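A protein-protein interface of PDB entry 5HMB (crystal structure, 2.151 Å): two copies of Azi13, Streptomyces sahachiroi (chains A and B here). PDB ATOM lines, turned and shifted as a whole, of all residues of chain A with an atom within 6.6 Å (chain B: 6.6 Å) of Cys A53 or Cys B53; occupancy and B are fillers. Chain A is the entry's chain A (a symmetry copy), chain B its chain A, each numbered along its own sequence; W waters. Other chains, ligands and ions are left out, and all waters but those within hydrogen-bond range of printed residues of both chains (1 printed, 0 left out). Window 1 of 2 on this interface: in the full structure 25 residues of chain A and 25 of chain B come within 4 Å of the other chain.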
ATOM      1  N   HIS A  48      36.967 -11.779  27.587  1.00  0.00           N
ATOM      2  CA  HIS A  48      35.574 -11.366  27.455  1.00  0.00           C
ATOM      3  C   HIS A  48      34.688 -12.599  27.339  1.00  0.00           C
ATOM      4  O   HIS A  48      35.018 -13.548  26.624  1.00  0.00           O
ATOM      5  CB  HIS A  48      35.429 -10.476  26.216  1.00  0.00           C
ATOM      6  CG  HIS A  48      34.148  -9.713  26.148  1.00  0.00           C
ATOM      7  ND1 HIS A  48      32.933 -10.312  25.876  1.00  0.00           N
ATOM      8  CD2 HIS A  48      33.895  -8.389  26.276  1.00  0.00           C
ATOM      9  CE1 HIS A  48      31.988  -9.390  25.850  1.00  0.00           C
ATOM     10  NE2 HIS A  48      32.544  -8.214  26.095  1.00  0.00           N
ATOM     11  N   GLY A  49      33.581 -12.601  28.081  1.00  0.00           N
ATOM     12  CA  GLY A  49      32.710 -13.760  28.092  1.00  0.00           C
ATOM     13  C   GLY A  49      32.069 -14.032  26.743  1.00  0.00           C
ATOM     14  O   GLY A  49      31.847 -15.185  26.388  1.00  0.00           O
ATOM     15  N   GLY A  50      31.749 -12.978  25.984  1.00  0.00           N
ATOM     16  CA  GLY A  50      31.197 -13.171  24.654  1.00  0.00           C
ATOM     17  C   GLY A  50      32.094 -13.990  23.752  1.00  0.00           C
ATOM     18  O   GLY A  50      31.605 -14.708  22.883  1.00  0.00           O
ATOM     19  N   VAL A  51      33.418 -13.920  23.956  1.00  0.00           N
ATOM     20  CA  VAL A  51      34.309 -14.738  23.139  1.00  0.00           C
ATOM     21  C   VAL A  51      34.036 -16.221  23.374  1.00  0.00           C
ATOM     22  O   VAL A  51      33.987 -17.011  22.427  1.00  0.00           O
ATOM     23  CB  VAL A  51      35.781 -14.380  23.411  1.00  0.00           C
ATOM     24  CG1 VAL A  51      36.680 -15.247  22.524  1.00  0.00           C
ATOM     25  CG2 VAL A  51      36.022 -12.901  23.139  1.00  0.00           C
ATOM     26  N   HIS A  52      33.845 -16.620  24.637  1.00  0.00           N
ATOM     27  CA  HIS A  52      33.476 -18.004  24.930  1.00  0.00           C
ATOM     28  C   HIS A  52      32.201 -18.405  24.198  1.00  0.00           C
ATOM     29  O   HIS A  52      32.129 -19.488  23.609  1.00  0.00           O
ATOM     30  CB  HIS A  52      33.300 -18.209  26.441  1.00  0.00           C
ATOM     31  CG  HIS A  52      34.582 -18.466  27.160  1.00  0.00           C
ATOM     32  ND1 HIS A  52      35.510 -19.380  26.711  1.00  0.00           N
ATOM     33  CD2 HIS A  52      35.094 -17.930  28.297  1.00  0.00           C
ATOM     34  CE1 HIS A  52      36.541 -19.393  27.539  1.00  0.00           C
ATOM     35  NE2 HIS A  52      36.310 -18.528  28.510  1.00  0.00           N
ATOM     36  N   CYS A  53      31.175 -17.552  24.245  1.00  0.00           N
ATOM     37  CA  CYS A  53      29.919 -17.860  23.555  1.00  0.00           C
ATOM     38  C   CYS A  53      30.124 -17.973  22.057  1.00  0.00           C
ATOM     39  O   CYS A  53      29.561 -18.866  21.410  1.00  0.00           O
ATOM     40  CB  CYS A  53      28.886 -16.775  23.828  1.00  0.00           C
ATOM     41  SG  CYS A  53      28.570 -16.447  25.607  1.00  0.00           S
ATOM     42  N   ALA A  54      30.895 -17.043  21.482  1.00  0.00           N
ATOM     43  CA  ALA A  54      31.129 -17.045  20.041  1.00  0.00           C
ATOM     44  C   ALA A  54      31.867 -18.303  19.593  1.00  0.00           C
ATOM     45  O   ALA A  54      31.581 -18.851  18.521  1.00  0.00           O
ATOM     46  CB  ALA A  54      31.913 -15.789  19.650  1.00  0.00           C
ATOM     47  N   VAL A  55      32.846 -18.754  20.381  1.00  0.00           N
ATOM     48  CA  VAL A  55      33.571 -19.980  20.049  1.00  0.00           C
ATOM     49  C   VAL A  55      32.656 -21.191  20.154  1.00  0.00           C
ATOM     50  O   VAL A  55      32.728 -22.124  19.342  1.00  0.00           O
ATOM     51  CB  VAL A  55      34.788 -20.141  20.975  1.00  0.00           C
ATOM     52  CG1 VAL A  55      35.324 -21.580  20.906  1.00  0.00           C
ATOM     53  CG2 VAL A  55      35.851 -19.129  20.615  1.00  0.00           C
ATOM     54  N   VAL A  56      31.827 -21.230  21.193  1.00  0.00           N
ATOM     55  CA  VAL A  56      30.850 -22.307  21.319  1.00  0.00           C
ATOM     56  C   VAL A  56      29.917 -22.315  20.106  1.00  0.00           C
ATOM     57  O   VAL A  56      29.666 -23.359  19.488  1.00  0.00           O
ATOM     58  CB  VAL A  56      30.088 -22.150  22.649  1.00  0.00           C
ATOM     59  CG1 VAL A  56      28.836 -22.987  22.657  1.00  0.00           C
ATOM     60  CG2 VAL A  56      30.988 -22.540  23.834  1.00  0.00           C
ATOM     61  N   GLU A  57      29.401 -21.142  19.739  1.00  0.00           N
ATOM     62  CA  GLU A  57      28.555 -21.046  18.554  1.00  0.00           C
ATOM     63  C   GLU A  57      29.291 -21.559  17.319  1.00  0.00           C
ATOM     64  O   GLU A  57      28.774 -22.414  16.585  1.00  0.00           O
ATOM     65  CB  GLU A  57      28.079 -19.599  18.366  1.00  0.00           C
ATOM     66  CG  GLU A  57      26.940 -19.479  17.319  1.00  0.00           C
ATOM     67  CD  GLU A  57      25.612 -20.020  17.848  1.00  0.00           C
ATOM     68  OE1 GLU A  57      25.403 -19.988  19.081  1.00  0.00           O
ATOM     69  OE2 GLU A  57      24.777 -20.476  17.043  1.00  0.00           O
ATOM     70  N   SER A  58      30.527 -21.088  17.101  1.00  0.00           N
ATOM     71  CA  SER A  58      31.297 -21.477  15.912  1.00  0.00           C
ATOM     72  C   SER A  58      31.534 -22.982  15.857  1.00  0.00           C
ATOM     73  O   SER A  58      31.365 -23.610  14.804  1.00  0.00           O
ATOM     74  CB  SER A  58      32.651 -20.759  15.890  1.00  0.00           C
ATOM     75  OG  SER A  58      32.546 -19.351  15.941  1.00  0.00           O
ATOM     76  N   SER A  78      19.665 -20.737  19.594  1.00  0.00           N
ATOM     77  CA  SER A  78      19.995 -20.246  20.930  1.00  0.00           C
ATOM     78  C   SER A  78      21.317 -20.830  21.393  1.00  0.00           C
ATOM     79  O   SER A  78      21.768 -21.871  20.912  1.00  0.00           O
ATOM     80  CB  SER A  78      18.912 -20.580  21.958  1.00  0.00           C
ATOM     81  OG  SER A  78      18.852 -21.968  22.212  1.00  0.00           O
ATOM     82  N   ASN A  79      21.894 -20.167  22.391  1.00  0.00           N
ATOM     83  CA  ASN A  79      23.246 -20.441  22.853  1.00  0.00           C
ATOM     84  C   ASN A  79      23.294 -20.130  24.343  1.00  0.00           C
ATOM     85  O   ASN A  79      23.129 -18.970  24.737  1.00  0.00           O
ATOM     86  CB  ASN A  79      24.243 -19.581  22.085  1.00  0.00           C
ATOM     87  CG  ASN A  79      25.668 -19.779  22.538  1.00  0.00           C
ATOM     88  OD1 ASN A  79      25.969 -19.796  23.742  1.00  0.00           O
ATOM     89  ND2 ASN A  79      26.573 -19.924  21.568  1.00  0.00           N
ATOM     90  N   SER A  80      23.554 -21.152  25.151  1.00  0.00           N
ATOM     91  CA  SER A  80      23.646 -21.015  26.601  1.00  0.00           C
ATOM     92  C   SER A  80      25.029 -21.482  27.030  1.00  0.00           C
ATOM     93  O   SER A  80      25.321 -22.682  26.985  1.00  0.00           O
ATOM     94  CB  SER A  80      22.558 -21.831  27.289  1.00  0.00           C
ATOM     95  OG  SER A  80      22.383 -21.404  28.619  1.00  0.00           O
ATOM     96  N   THR A  81      25.872 -20.543  27.450  1.00  0.00           N
ATOM     97  CA  THR A  81      27.258 -20.835  27.793  1.00  0.00           C
ATOM     98  C   THR A  81      27.512 -20.457  29.247  1.00  0.00           C
ATOM     99  O   THR A  81      27.140 -19.358  29.679  1.00  0.00           O
ATOM    100  CB  THR A  81      28.222 -20.101  26.851  1.00  0.00           C
ATOM    101  OG1 THR A  81      28.062 -20.588  25.503  1.00  0.00           O
ATOM    102  CG2 THR A  81      29.686 -20.292  27.264  1.00  0.00           C
ATOM    103  N   PHE A  83      30.569 -19.910  32.080  1.00  0.00           N
ATOM    104  CA  PHE A  83      31.992 -19.632  32.213  1.00  0.00           C
ATOM    105  C   PHE A  83      32.414 -20.112  33.593  1.00  0.00           C
ATOM    106  O   PHE A  83      31.911 -19.601  34.598  1.00  0.00           O
ATOM    107  CB  PHE A  83      32.286 -18.142  32.038  1.00  0.00           C
ATOM    108  CG  PHE A  83      31.383 -17.458  31.063  1.00  0.00           C
ATOM    109  CD1 PHE A  83      31.434 -17.773  29.708  1.00  0.00           C
ATOM    110  CD2 PHE A  83      30.497 -16.476  31.487  1.00  0.00           C
ATOM    111  CE1 PHE A  83      30.597 -17.140  28.788  1.00  0.00           C
ATOM    112  CE2 PHE A  83      29.659 -15.831  30.572  1.00  0.00           C
ATOM    113  CZ  PHE A  83      29.709 -16.173  29.215  1.00  0.00           C
ATOM    114  N   ALA A 123      34.966 -23.332  30.026  1.00  0.00           N
ATOM    115  CA  ALA A 123      33.641 -22.865  29.650  1.00  0.00           C
ATOM    116  C   ALA A 123      32.931 -24.016  28.970  1.00  0.00           C
ATOM    117  O   ALA A 123      33.571 -24.947  28.476  1.00  0.00           O
ATOM    118  CB  ALA A 123      33.705 -21.640  28.728  1.00  0.00           C
ATOM    119  N   VAL A 127      24.152 -25.428  22.286  1.00  0.00           N
ATOM    120  CA  VAL A 127      23.760 -24.663  21.108  1.00  0.00           C
ATOM    121  C   VAL A 127      22.624 -25.401  20.400  1.00  0.00           C
ATOM    122  O   VAL A 127      22.776 -26.563  19.992  1.00  0.00           O
ATOM    123  CB  VAL A 127      24.942 -24.429  20.155  1.00  0.00           C
ATOM    124  CG1 VAL A 127      24.482 -23.745  18.888  1.00  0.00           C
ATOM    125  CG2 VAL A 127      25.966 -23.571  20.825  1.00  0.00           C
ATOM    126  N   HIS B  48      26.923 -13.454  12.617  1.00  0.00           N
ATOM    127  CA  HIS B  48      27.364 -14.556  13.465  1.00  0.00           C
ATOM    128  C   HIS B  48      26.631 -14.495  14.798  1.00  0.00           C
ATOM    129  O   HIS B  48      26.475 -13.421  15.384  1.00  0.00           O
ATOM    130  CB  HIS B  48      28.878 -14.455  13.674  1.00  0.00           C
ATOM    131  CG  HIS B  48      29.511 -15.688  14.230  1.00  0.00           C
ATOM    132  ND1 HIS B  48      29.344 -16.089  15.541  1.00  0.00           N
ATOM    133  CD2 HIS B  48      30.347 -16.590  13.664  1.00  0.00           C
ATOM    134  CE1 HIS B  48      30.042 -17.189  15.753  1.00  0.00           C
ATOM    135  NE2 HIS B  48      30.656 -17.518  14.628  1.00  0.00           N
ATOM    136  N   GLY B  49      26.143 -15.648  15.255  1.00  0.00           N
ATOM    137  CA  GLY B  49      25.370 -15.680  16.481  1.00  0.00           C
ATOM    138  C   GLY B  49      26.179 -15.286  17.703  1.00  0.00           C
ATOM    139  O   GLY B  49      25.645 -14.680  18.627  1.00  0.00           O
ATOM    140  N   GLY B  50      27.469 -15.637  17.733  1.00  0.00           N
ATOM    141  CA  GLY B  50      28.316 -15.230  18.841  1.00  0.00           C
ATOM    142  C   GLY B  50      28.360 -13.730  19.036  1.00  0.00           C
ATOM    143  O   GLY B  50      28.509 -13.259  20.161  1.00  0.00           O
ATOM    144  N   VAL B  51      28.205 -12.954  17.954  1.00  0.00           N
ATOM    145  CA  VAL B  51      28.188 -11.504  18.112  1.00  0.00           C
ATOM    146  C   VAL B  51      27.004 -11.076  18.974  1.00  0.00           C
ATOM    147  O   VAL B  51      27.140 -10.222  19.855  1.00  0.00           O
ATOM    148  CB  VAL B  51      28.177 -10.803  16.742  1.00  0.00           C
ATOM    149  CG1 VAL B  51      28.177  -9.286  16.953  1.00  0.00           C
ATOM    150  CG2 VAL B  51      29.388 -11.233  15.923  1.00  0.00           C
ATOM    151  N   HIS B  52      25.826 -11.667  18.740  1.00  0.00           N
ATOM    152  CA  HIS B  52      24.672 -11.386  19.592  1.00  0.00           C
ATOM    153  C   HIS B  52      24.976 -11.688  21.054  1.00  0.00           C
ATOM    154  O   HIS B  52      24.652 -10.891  21.941  1.00  0.00           O
ATOM    155  CB  HIS B  52      23.450 -12.193  19.132  1.00  0.00           C
ATOM    156  CG  HIS B  52      22.699 -11.551  18.014  1.00  0.00           C
ATOM    157  ND1 HIS B  52      22.350 -10.219  18.028  1.00  0.00           N
ATOM    158  CD2 HIS B  52      22.231 -12.056  16.844  1.00  0.00           C
ATOM    159  CE1 HIS B  52      21.700  -9.929  16.913  1.00  0.00           C
ATOM    160  NE2 HIS B  52      21.611 -11.026  16.182  1.00  0.00           N
ATOM    161  N   CYS B  53      25.576 -12.849  21.327  1.00  0.00           N
ATOM    162  CA  CYS B  53      25.913 -13.206  22.708  1.00  0.00           C
ATOM    163  C   CYS B  53      26.905 -12.227  23.307  1.00  0.00           C
ATOM    164  O   CYS B  53      26.776 -11.835  24.474  1.00  0.00           O
ATOM    165  CB  CYS B  53      26.513 -14.604  22.761  1.00  0.00           C
ATOM    166  SG  CYS B  53      25.473 -15.914  22.002  1.00  0.00           S
ATOM    167  N   ALA B  54      27.930 -11.857  22.532  1.00  0.00           N
ATOM    168  CA  ALA B  54      28.956 -10.943  23.025  1.00  0.00           C
ATOM    169  C   ALA B  54      28.375  -9.571  23.354  1.00  0.00           C
ATOM    170  O   ALA B  54      28.779  -8.938  24.338  1.00  0.00           O
ATOM    171  CB  ALA B  54      30.074 -10.822  21.986  1.00  0.00           C
ATOM    172  N   VAL B  55      27.453  -9.078  22.523  1.00  0.00           N
ATOM    173  CA  VAL B  55      26.812  -7.792  22.793  1.00  0.00           C
ATOM    174  C   VAL B  55      25.936  -7.877  24.033  1.00  0.00           C
ATOM    175  O   VAL B  55      25.871  -6.939  24.841  1.00  0.00           O
ATOM    176  CB  VAL B  55      25.982  -7.352  21.576  1.00  0.00           C
ATOM    177  CG1 VAL B  55      25.011  -6.226  21.972  1.00  0.00           C
ATOM    178  CG2 VAL B  55      26.897  -6.931  20.449  1.00  0.00           C
ATOM    179  N   VAL B  56      25.197  -8.974  24.174  1.00  0.00           N
ATOM    180  CA  VAL B  56      24.402  -9.179  25.381  1.00  0.00           C
ATOM    181  C   VAL B  56      25.309  -9.190  26.613  1.00  0.00           C
ATOM    182  O   VAL B  56      25.041  -8.521  27.621  1.00  0.00           O
ATOM    183  CB  VAL B  56      23.586 -10.478  25.237  1.00  0.00           C
ATOM    184  CG1 VAL B  56      23.053 -10.933  26.571  1.00  0.00           C
ATOM    185  CG2 VAL B  56      22.424 -10.278  24.249  1.00  0.00           C
ATOM    186  N   GLU B  57      26.408  -9.941  26.542  1.00  0.00           N
ATOM    187  CA  GLU B  57      27.364  -9.958  27.644  1.00  0.00           C
ATOM    188  C   GLU B  57      27.866  -8.548  27.948  1.00  0.00           C
ATOM    189  O   GLU B  57      27.823  -8.098  29.103  1.00  0.00           O
ATOM    190  CB  GLU B  57      28.522 -10.910  27.319  1.00  0.00           C
ATOM    191  CG  GLU B  57      29.407 -11.214  28.557  1.00  0.00           C
ATOM    192  CD  GLU B  57      28.708 -12.140  29.552  1.00  0.00           C
ATOM    193  OE1 GLU B  57      27.852 -12.943  29.120  1.00  0.00           O
ATOM    194  OE2 GLU B  57      29.008 -12.072  30.760  1.00  0.00           O
ATOM    195  N   SER B  58      28.296  -7.813  26.913  1.00  0.00           N
ATOM    196  CA  SER B  58      28.849  -6.467  27.107  1.00  0.00           C
ATOM    197  C   SER B  58      27.836  -5.523  27.746  1.00  0.00           C
ATOM    198  O   SER B  58      28.166  -4.779  28.678  1.00  0.00           O
ATOM    199  CB  SER B  58      29.305  -5.874  25.769  1.00  0.00           C
ATOM    200  OG  SER B  58      30.248  -6.676  25.087  1.00  0.00           O
ATOM    201  N   SER B  78      27.210 -16.813  33.405  1.00  0.00           N
ATOM    202  CA  SER B  78      26.574 -17.525  32.298  1.00  0.00           C
ATOM    203  C   SER B  78      25.780 -16.560  31.439  1.00  0.00           C
ATOM    204  O   SER B  78      25.385 -15.477  31.878  1.00  0.00           O
ATOM    205  CB  SER B  78      25.649 -18.645  32.781  1.00  0.00           C
ATOM    206  OG  SER B  78      24.507 -18.127  33.431  1.00  0.00           O
ATOM    207  N   ASN B  79      25.496 -17.010  30.220  1.00  0.00           N
ATOM    208  CA  ASN B  79      24.916 -16.177  29.178  1.00  0.00           C
ATOM    209  C   ASN B  79      24.057 -17.075  28.298  1.00  0.00           C
ATOM    210  O   ASN B  79      24.584 -17.973  27.632  1.00  0.00           O
ATOM    211  CB  ASN B  79      26.022 -15.515  28.365  1.00  0.00           C
ATOM    212  CG  ASN B  79      25.498 -14.665  27.235  1.00  0.00           C
ATOM    213  OD1 ASN B  79      24.606 -15.075  26.474  1.00  0.00           O
ATOM    214  ND2 ASN B  79      26.057 -13.460  27.104  1.00  0.00           N
ATOM    215  N   SER B  80      22.756 -16.807  28.272  1.00  0.00           N
ATOM    216  CA  SER B  80      21.803 -17.567  27.470  1.00  0.00           C
ATOM    217  C   SER B  80      21.112 -16.599  26.521  1.00  0.00           C
ATOM    218  O   SER B  80      20.300 -15.775  26.956  1.00  0.00           O
ATOM    219  CB  SER B  80      20.789 -18.273  28.362  1.00  0.00           C
ATOM    220  OG  SER B  80      20.135 -19.299  27.656  1.00  0.00           O
ATOM    221  N   THR B  81      21.424 -16.702  25.232  1.00  0.00           N
ATOM    222  CA  THR B  81      20.915 -15.775  24.229  1.00  0.00           C
ATOM    223  C   THR B  81      20.121 -16.545  23.182  1.00  0.00           C
ATOM    224  O   THR B  81      20.587 -17.576  22.679  1.00  0.00           O
ATOM    225  CB  THR B  81      22.061 -14.982  23.585  1.00  0.00           C
ATOM    226  OG1 THR B  81      22.701 -14.148  24.573  1.00  0.00           O
ATOM    227  CG2 THR B  81      21.568 -14.087  22.441  1.00  0.00           C
ATOM    228  N   PHE B  83      18.329 -16.175  19.398  1.00  0.00           N
ATOM    229  CA  PHE B  83      18.365 -15.397  18.167  1.00  0.00           C
ATOM    230  C   PHE B  83      17.021 -15.585  17.480  1.00  0.00           C
ATOM    231  O   PHE B  83      16.673 -16.711  17.115  1.00  0.00           O
ATOM    232  CB  PHE B  83      19.511 -15.846  17.260  1.00  0.00           C
ATOM    233  CG  PHE B  83      20.725 -16.304  18.000  1.00  0.00           C
ATOM    234  CD1 PHE B  83      21.480 -15.405  18.749  1.00  0.00           C
ATOM    235  CD2 PHE B  83      21.139 -17.628  17.932  1.00  0.00           C
ATOM    236  CE1 PHE B  83      22.617 -15.821  19.444  1.00  0.00           C
ATOM    237  CE2 PHE B  83      22.280 -18.054  18.619  1.00  0.00           C
ATOM    238  CZ  PHE B  83      23.017 -17.141  19.384  1.00  0.00           C
ATOM    239  N   ALA B 123      17.249 -10.353  18.958  1.00  0.00           N
ATOM    240  CA  ALA B 123      17.900 -11.308  19.841  1.00  0.00           C
ATOM    241  C   ALA B 123      17.622 -10.871  21.263  1.00  0.00           C
ATOM    242  O   ALA B 123      17.304  -9.707  21.514  1.00  0.00           O
ATOM    243  CB  ALA B 123      19.409 -11.394  19.579  1.00  0.00           C
ATOM    244  N   VAL B 127      21.830 -12.768  31.384  1.00  0.00           N
ATOM    245  CA  VAL B 127      23.225 -12.807  31.808  1.00  0.00           C
ATOM    246  C   VAL B 127      23.271 -12.858  33.335  1.00  0.00           C
ATOM    247  O   VAL B 127      22.754 -11.961  34.018  1.00  0.00           O
ATOM    248  CB  VAL B 127      24.022 -11.608  31.273  1.00  0.00           C
ATOM    249  CG1 VAL B 127      25.428 -11.608  31.829  1.00  0.00           C
ATOM    250  CG2 VAL B 127      24.090 -11.676  29.782  1.00  0.00           C
HETATM  251  O   HOH W   1      25.586 -17.220  24.884  1.00  0.00           O
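The backbone NH of Thr B81 lies within hydrogen-bond range of the backbone carbonyl oxygen of Asn A79.
A ring nitrogen (NE2) of His B48 is in hydrogen-bond range of the side-chain hydroxyl (OG) of Ser A58, 2.9 Å away.
O of Asn B79 sits close to O of Asn A79 (3.4 Å).
N of Thr A81 sits at hydrogen-bond distance from O of Asn B79, at 2.9 Å.
OG of Ser B58 is in hydrogen-bond range of NE2 of His A48 (2.9 Å).
OG of Ser B80 is in hydrogen-bond range of OG of Ser A80.
ND1 of His A48 sits at hydrogen-bond distance from N of Gly A50, at 2.9 Å.
N of Gly B50 lies within hydrogen-bond range of ND1 of His B48, at 2.9 Å.
The side-chain carboxylate (OE1) of Glu B57 lies within hydrogen-bond range of the side-chain amide nitrogen (ND2) of Asn B79 (2.7 Å).
The backbone carbonyl oxygen (O) of Cys A53 lies within hydrogen-bond range of the side-chain amide nitrogen (ND2) of Asn A79 (3.2 Å).
The side-chain amide oxygen of Asn A79 lies within hydrogen-bond range of the side-chain hydroxyl of Thr A81 (2.8 Å).
OG of Ser A58 lies within hydrogen-bond range of O of Ala A54, at 2.8 Å.
Among the printed residues, pairs that only touch across the chains: Ser A78 with Thr B81 (3.2 Å), Thr A81 with Ser B78 (3.2 Å), Asn A79 with Ser B80 (3.3 Å), Ser A80 with Asn B79 (3.3 Å), Cys A53 with Cys B53 (3.4 Å), Gly A50 with Ala B54 (3.6 Å), Ala A54 with Gly B50 (3.6 Å), His A48 with Ala B54 (3.6 Å), Ala A54 with His B48 (3.6 Å), Glu A57 with Phe B83 (3.7 Å), Phe A83 with Glu B57 (3.7 Å), Phe A83 with Ser B78 (3.8 Å), Ser A78 with Phe B83 (3.8 Å), Phe A83 with Asn B79 (3.8 Å), Asn A79 with Phe B83 (3.8 Å), Asn A79 with Cys B53 (3.9 Å), Cys A53 with Asn B79 (3.9 Å), Glu A57 with Gly B50 (3.9 Å) and Gly A50 with Glu B57 (3.9 Å).
Of chain B, only Cys B53 (3.4 Å) and Asn B79 (3.9 Å) come within 4 Å of Cys A53.
Printed residues of chain B within 4 Å of Glu A57: Gly B50 (3.9 Å) and Phe B83 (3.7 Å).
Printed residues of chain B within 4 Å of Ser A58: His B48 (2.9 Å).
Cys B53 touches two residues of chain A.
Printed residues of chain A within 4 Å of Ser B80: Asn A79 and Ser A80.
The nearest printed residue of chain B that does not touch Ala A54 is Val B51 (5.0 Å).
Of the 18 printed residues of chain B, 11 touch a printed residue of chain A.
Hydrophobic or aromatic side chains of chain B within 4 Å of the printed part of chain A: His B48, Ala B54 and Phe B83.
Hydrophobic or aromatic side chains of chain A within 4 Å of the printed part of chain B: His A48, Ala A54 and Phe A83.
His A48 touches Ala B54, and with the chains exchanged Ala A54 touches His B48.
Gly A50 touches Ala B54, and with the chains exchanged Ala A54 touches Gly B50.
Cys A53 touches its own counterpart, Cys B53.
Asn A79 touches Ser B80, and with the chains exchanged Ser A80 touches Asn B79.
Positions printed for both chains: 48, 49, 50, 51, 52, 53, 54, 55, 56, 57, 58, 78, 79, 80, 81, 83, 123 and 127.
Water W1 lies within hydrogen-bond range of the side-chain amide oxygen (OD1) of Asn B79 (2.8 Å), the side-chain amide oxygen (OD1) of Asn A79 (2.8 Å), the side-chain sulfur (SG) of Cys B53 (3.2 Å) and the side-chain sulfur (SG) of Cys A53 (3.2 Å).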
